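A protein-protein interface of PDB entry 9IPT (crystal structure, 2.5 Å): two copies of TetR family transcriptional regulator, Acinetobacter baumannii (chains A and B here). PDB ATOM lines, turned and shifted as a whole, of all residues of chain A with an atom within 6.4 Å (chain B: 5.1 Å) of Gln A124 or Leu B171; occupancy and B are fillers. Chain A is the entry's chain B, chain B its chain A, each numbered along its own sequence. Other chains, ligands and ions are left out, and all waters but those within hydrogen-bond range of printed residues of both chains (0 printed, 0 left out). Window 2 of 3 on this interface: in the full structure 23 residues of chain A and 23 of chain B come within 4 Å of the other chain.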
ATOM      1  N   TYR A 119      20.651  12.930   2.988  1.00  0.00           N
ATOM      2  CA  TYR A 119      19.747  11.817   2.719  1.00  0.00           C
ATOM      3  C   TYR A 119      18.321  12.157   3.134  1.00  0.00           C
ATOM      4  O   TYR A 119      17.369  11.896   2.390  1.00  0.00           O
ATOM      5  CB  TYR A 119      20.233  10.556   3.436  1.00  0.00           C
ATOM      6  CG  TYR A 119      19.417   9.326   3.106  1.00  0.00           C
ATOM      7  CD1 TYR A 119      19.726   8.541   2.003  1.00  0.00           C
ATOM      8  CD2 TYR A 119      18.333   8.956   3.891  1.00  0.00           C
ATOM      9  CE1 TYR A 119      18.980   7.419   1.695  1.00  0.00           C
ATOM     10  CE2 TYR A 119      17.581   7.838   3.589  1.00  0.00           C
ATOM     11  CZ  TYR A 119      17.909   7.073   2.491  1.00  0.00           C
ATOM     12  OH  TYR A 119      17.161   5.959   2.189  1.00  0.00           O
ATOM     13  N   ASN A 120      18.153  12.737   4.325  1.00  0.00           N
ATOM     14  CA  ASN A 120      16.820  13.126   4.772  1.00  0.00           C
ATOM     15  C   ASN A 120      16.244  14.240   3.911  1.00  0.00           C
ATOM     16  O   ASN A 120      15.024  14.309   3.724  1.00  0.00           O
ATOM     17  CB  ASN A 120      16.862  13.555   6.238  1.00  0.00           C
ATOM     18  CG  ASN A 120      16.837  12.376   7.191  1.00  0.00           C
ATOM     19  OD1 ASN A 120      17.072  11.236   6.791  1.00  0.00           O
ATOM     20  ND2 ASN A 120      16.553  12.646   8.459  1.00  0.00           N
ATOM     21  N   LEU A 121      17.099  15.116   3.379  1.00  0.00           N
ATOM     22  CA  LEU A 121      16.618  16.177   2.502  1.00  0.00           C
ATOM     23  C   LEU A 121      16.092  15.609   1.189  1.00  0.00           C
ATOM     24  O   LEU A 121      15.029  16.020   0.709  1.00  0.00           O
ATOM     25  CB  LEU A 121      17.734  17.188   2.243  1.00  0.00           C
ATOM     26  CG  LEU A 121      17.618  18.527   2.969  1.00  0.00           C
ATOM     27  CD1 LEU A 121      17.357  18.315   4.453  1.00  0.00           C
ATOM     28  CD2 LEU A 121      18.875  19.355   2.757  1.00  0.00           C
ATOM     29  N   ALA A 122      16.823  14.663   0.595  1.00  0.00           N
ATOM     30  CA  ALA A 122      16.361  14.036  -0.639  1.00  0.00           C
ATOM     31  C   ALA A 122      15.084  13.240  -0.405  1.00  0.00           C
ATOM     32  O   ALA A 122      14.197  13.203  -1.266  1.00  0.00           O
ATOM     33  CB  ALA A 122      17.456  13.139  -1.214  1.00  0.00           C
ATOM     34  N   MET A 123      14.973  12.594   0.759  1.00  0.00           N
ATOM     35  CA  MET A 123      13.758  11.854   1.083  1.00  0.00           C
ATOM     36  C   MET A 123      12.575  12.796   1.270  1.00  0.00           C
ATOM     37  O   MET A 123      11.441  12.457   0.913  1.00  0.00           O
ATOM     38  CB  MET A 123      13.982  11.007   2.336  1.00  0.00           C
ATOM     39  CG  MET A 123      14.493   9.602   2.049  1.00  0.00           C
ATOM     40  SD  MET A 123      13.167   8.385   1.948  1.00  0.00           S
ATOM     41  CE  MET A 123      14.083   6.914   1.496  1.00  0.00           C
ATOM     42  N   GLN A 124      12.820  13.986   1.826  1.00  0.00           N
ATOM     43  CA  GLN A 124      11.753  14.974   1.947  1.00  0.00           C
ATOM     44  C   GLN A 124      11.356  15.537   0.590  1.00  0.00           C
ATOM     45  O   GLN A 124      10.182  15.860   0.373  1.00  0.00           O
ATOM     46  CB  GLN A 124      12.180  16.099   2.890  1.00  0.00           C
ATOM     47  CG  GLN A 124      11.754  15.887   4.333  1.00  0.00           C
ATOM     48  CD  GLN A 124      12.740  16.473   5.325  1.00  0.00           C
ATOM     49  OE1 GLN A 124      13.548  15.755   5.913  1.00  0.00           O
ATOM     50  NE2 GLN A 124      12.676  17.786   5.516  1.00  0.00           N
ATOM     51  N   SER A 125      12.313  15.668  -0.333  1.00  0.00           N
ATOM     52  CA  SER A 125      11.970  16.073  -1.692  1.00  0.00           C
ATOM     53  C   SER A 125      11.267  14.950  -2.443  1.00  0.00           C
ATOM     54  O   SER A 125      10.401  15.216  -3.285  1.00  0.00           O
ATOM     55  CB  SER A 125      13.225  16.514  -2.444  1.00  0.00           C
ATOM     56  OG  SER A 125      13.154  17.886  -2.789  1.00  0.00           O
ATOM     57  N   TRP A 126      11.629  13.697  -2.157  1.00  0.00           N
ATOM     58  CA  TRP A 126      10.933  12.562  -2.757  1.00  0.00           C
ATOM     59  C   TRP A 126       9.478  12.521  -2.309  1.00  0.00           C
ATOM     60  O   TRP A 126       8.568  12.321  -3.123  1.00  0.00           O
ATOM     61  CB  TRP A 126      11.648  11.262  -2.390  1.00  0.00           C
ATOM     62  CG  TRP A 126      11.193  10.072  -3.175  1.00  0.00           C
ATOM     63  CD1 TRP A 126      10.632  10.074  -4.418  1.00  0.00           C
ATOM     64  CD2 TRP A 126      11.261   8.699  -2.768  1.00  0.00           C
ATOM     65  NE1 TRP A 126      10.347   8.788  -4.812  1.00  0.00           N
ATOM     66  CE2 TRP A 126      10.724   7.926  -3.816  1.00  0.00           C
ATOM     67  CE3 TRP A 126      11.725   8.050  -1.620  1.00  0.00           C
ATOM     68  CZ2 TRP A 126      10.637   6.536  -3.750  1.00  0.00           C
ATOM     69  CZ3 TRP A 126      11.638   6.671  -1.556  1.00  0.00           C
ATOM     70  CH2 TRP A 126      11.098   5.929  -2.614  1.00  0.00           C
ATOM     71  N   HIS A 127       9.240  12.710  -1.009  1.00  0.00           N
ATOM     72  CA  HIS A 127       7.875  12.751  -0.498  1.00  0.00           C
ATOM     73  C   HIS A 127       7.103  13.934  -1.066  1.00  0.00           C
ATOM     74  O   HIS A 127       5.881  13.854  -1.236  1.00  0.00           O
ATOM     75  CB  HIS A 127       7.896  12.809   1.029  1.00  0.00           C
ATOM     76  CG  HIS A 127       6.540  12.915   1.650  1.00  0.00           C
ATOM     77  ND1 HIS A 127       6.016  14.110   2.094  1.00  0.00           N
ATOM     78  CD2 HIS A 127       5.602  11.974   1.907  1.00  0.00           C
ATOM     79  CE1 HIS A 127       4.812  13.900   2.595  1.00  0.00           C
ATOM     80  NE2 HIS A 127       4.536  12.613   2.493  1.00  0.00           N
ATOM     81  N   GLN A 128       7.797  15.033  -1.364  1.00  0.00           N
ATOM     82  CA  GLN A 128       7.145  16.191  -1.965  1.00  0.00           C
ATOM     83  C   GLN A 128       6.605  15.859  -3.350  1.00  0.00           C
ATOM     84  O   GLN A 128       5.453  16.172  -3.674  1.00  0.00           O
ATOM     85  CB  GLN A 128       8.130  17.357  -2.041  1.00  0.00           C
ATOM     86  CG  GLN A 128       7.804  18.523  -1.129  1.00  0.00           C
ATOM     87  CD  GLN A 128       8.649  19.744  -1.436  1.00  0.00           C
ATOM     88  OE1 GLN A 128       9.150  19.903  -2.550  1.00  0.00           O
ATOM     89  NE2 GLN A 128       8.813  20.615  -0.448  1.00  0.00           N
ATOM     90  N   ALA A 129       7.430  15.221  -4.183  1.00  0.00           N
ATOM     91  CA  ALA A 129       7.029  14.939  -5.558  1.00  0.00           C
ATOM     92  C   ALA A 129       5.883  13.937  -5.609  1.00  0.00           C
ATOM     93  O   ALA A 129       4.968  14.077  -6.429  1.00  0.00           O
ATOM     94  CB  ALA A 129       8.226  14.427  -6.358  1.00  0.00           C
ATOM     95  N   TRP A 154       3.550   8.946   2.190  1.00  0.00           N
ATOM     96  CA  TRP A 154       4.395   8.288   3.181  1.00  0.00           C
ATOM     97  C   TRP A 154       4.211   6.777   3.138  1.00  0.00           C
ATOM     98  O   TRP A 154       5.177   6.020   3.295  1.00  0.00           O
ATOM     99  CB  TRP A 154       4.085   8.826   4.577  1.00  0.00           C
ATOM    100  CG  TRP A 154       4.754  10.134   4.897  1.00  0.00           C
ATOM    101  CD1 TRP A 154       4.149  11.271   5.350  1.00  0.00           C
ATOM    102  CD2 TRP A 154       6.153  10.437   4.803  1.00  0.00           C
ATOM    103  NE1 TRP A 154       5.081  12.263   5.536  1.00  0.00           N
ATOM    104  CE2 TRP A 154       6.318  11.777   5.208  1.00  0.00           C
ATOM    105  CE3 TRP A 154       7.282   9.707   4.412  1.00  0.00           C
ATOM    106  CZ2 TRP A 154       7.564  12.401   5.234  1.00  0.00           C
ATOM    107  CZ3 TRP A 154       8.517  10.330   4.438  1.00  0.00           C
ATOM    108  CH2 TRP A 154       8.649  11.663   4.846  1.00  0.00           C
ATOM    109  N   ILE B 166      11.606   3.824   7.950  1.00  0.00           N
ATOM    110  CA  ILE B 166      11.427   5.258   7.762  1.00  0.00           C
ATOM    111  C   ILE B 166      11.368   5.985   9.099  1.00  0.00           C
ATOM    112  O   ILE B 166      11.661   7.186   9.168  1.00  0.00           O
ATOM    113  CB  ILE B 166      10.167   5.540   6.919  1.00  0.00           C
ATOM    114  CG1 ILE B 166      10.129   4.614   5.703  1.00  0.00           C
ATOM    115  CG2 ILE B 166      10.127   6.996   6.476  1.00  0.00           C
ATOM    116  CD1 ILE B 166      10.841   5.157   4.486  1.00  0.00           C
ATOM    117  N   LEU B 169      14.985   7.158  10.454  1.00  0.00           N
ATOM    118  CA  LEU B 169      15.698   8.265   9.828  1.00  0.00           C
ATOM    119  C   LEU B 169      15.485   9.594  10.535  1.00  0.00           C
ATOM    120  O   LEU B 169      16.158  10.570  10.189  1.00  0.00           O
ATOM    121  CB  LEU B 169      15.281   8.404   8.363  1.00  0.00           C
ATOM    122  CG  LEU B 169      15.265   7.128   7.521  1.00  0.00           C
ATOM    123  CD1 LEU B 169      14.136   7.170   6.502  1.00  0.00           C
ATOM    124  CD2 LEU B 169      16.610   6.912   6.843  1.00  0.00           C
ATOM    125  N   GLY B 170      14.576   9.664  11.502  1.00  0.00           N
ATOM    126  CA  GLY B 170      14.292  10.941  12.134  1.00  0.00           C
ATOM    127  C   GLY B 170      13.680  11.945  11.182  1.00  0.00           C
ATOM    128  O   GLY B 170      13.974  13.145  11.269  1.00  0.00           O
ATOM    129  N   LEU B 171      12.832  11.478  10.270  1.00  0.00           N
ATOM    130  CA  LEU B 171      12.257  12.343   9.252  1.00  0.00           C
ATOM    131  C   LEU B 171      11.336  13.386   9.876  1.00  0.00           C
ATOM    132  O   LEU B 171      10.630  13.123  10.853  1.00  0.00           O
ATOM    133  CB  LEU B 171      11.483  11.514   8.226  1.00  0.00           C
ATOM    134  CG  LEU B 171      11.913  11.604   6.758  1.00  0.00           C
ATOM    135  CD1 LEU B 171      13.127  12.508   6.581  1.00  0.00           C
ATOM    136  CD2 LEU B 171      12.181  10.219   6.188  1.00  0.00           C
ATOM    137  N   GLN B 172      11.354  14.582   9.298  1.00  0.00           N
ATOM    138  CA  GLN B 172      10.492  15.666   9.739  1.00  0.00           C
ATOM    139  C   GLN B 172       9.165  15.614   8.995  1.00  0.00           C
ATOM    140  O   GLN B 172       9.110  15.251   7.815  1.00  0.00           O
ATOM    141  CB  GLN B 172      11.163  17.024   9.517  1.00  0.00           C
ATOM    142  CG  GLN B 172      10.463  18.261  10.122  1.00  0.00           C
ATOM    143  CD  GLN B 172       9.788  18.037  11.476  1.00  0.00           C
ATOM    144  OE1 GLN B 172       8.877  17.218  11.619  1.00  0.00           O
ATOM    145  NE2 GLN B 172      10.240  18.779  12.481  1.00  0.00           N
ATOM    146  N   GLY B 173       8.097  15.990   9.693  1.00  0.00           N
ATOM    147  CA  GLY B 173       6.756  15.880   9.181  1.00  0.00           C
ATOM    148  C   GLY B 173       6.087  14.561   9.503  1.00  0.00           C
ATOM    149  O   GLY B 173       4.870  14.526   9.704  1.00  0.00           O
ATOM    150  N   LEU B 174       6.852  13.478   9.565  1.00  0.00           N
ATOM    151  CA  LEU B 174       6.279  12.180   9.869  1.00  0.00           C
ATOM    152  C   LEU B 174       6.089  12.067  11.378  1.00  0.00           C
ATOM    153  O   LEU B 174       6.899  12.573  12.162  1.00  0.00           O
ATOM    154  CB  LEU B 174       7.189  11.059   9.366  1.00  0.00           C
ATOM    155  CG  LEU B 174       6.520   9.818   8.761  1.00  0.00           C
ATOM    156  CD1 LEU B 174       7.560   8.939   8.035  1.00  0.00           C
ATOM    157  CD2 LEU B 174       5.632   9.021   9.736  1.00  0.00           C
ATOM    158  N   GLU B 176       5.602   9.467  14.642  1.00  0.00           N
ATOM    159  CA  GLU B 176       5.762   8.104  15.134  1.00  0.00           C
ATOM    160  C   GLU B 176       4.525   7.593  15.859  1.00  0.00           C
ATOM    161  O   GLU B 176       4.434   6.389  16.123  1.00  0.00           O
ATOM    162  CB  GLU B 176       6.980   8.008  16.061  1.00  0.00           C
ATOM    163  CG  GLU B 176       8.327   8.180  15.364  1.00  0.00           C
ATOM    164  CD  GLU B 176       8.610   9.618  14.968  1.00  0.00           C
ATOM    165  OE1 GLU B 176       8.807   9.875  13.763  1.00  0.00           O
ATOM    166  OE2 GLU B 176       8.633  10.491  15.862  1.00  0.00           O
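Of chain B, only Leu B171 comes within 4 Å of Gln A124. Leu B171 touches just these residues of chain A: Asn A120, Gln A124 and Trp A154. Printed residues of chain B within 4 Å of Asn A120: Leu B169 (2.7 Å), Gly B170 (3.8 Å) and Leu B171 (3.8 Å). Printed residues of chain B within 4 Å of Tyr A119: Leu B169. Of the printed residues of chain B, Trp A154 touches Leu B171 (3.8 Å) and Leu B174 (3.7 Å). Printed residues of chain A within 4 Å of Leu B174: Trp A154 (3.7 Å). Gly B173 touches none of the printed residues of chain A. The nearest residue of chain B that does not touch Gln A124 is Gln B172 (4.2 Å).
The backbone carbonyl oxygen of Leu B169 sits at hydrogen-bond distance from the side-chain amide nitrogen of Asn A120 (2.7 Å).
No position is printed for both chains. Of the 7 pairs that touch across the chains among the printed residues, none has its exchanged pair printed and touching as well.
NE2 of His A127 lies within hydrogen-bond range of NE1 of Trp A154. The side-chain amide oxygen (OE1) of Gln A124 lies close to the backbone carbonyl oxygen (O) of Asn A120, at 3.0 Å.
Of the 8 printed residues of chain B, 4 touch a printed residue of chain A.
Among the printed residues, pairs that only touch across the chains: Gln A124 with Leu B171 (3.3 Å), Tyr A119 with Leu B169 (3.5 Å), Trp A154 with Leu B174 (3.7 Å), Asn A120 with Leu B171 (3.8 Å), Trp A154 with Leu B171 (3.8 Å) and Asn A120 with Gly B170 (3.8 Å).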
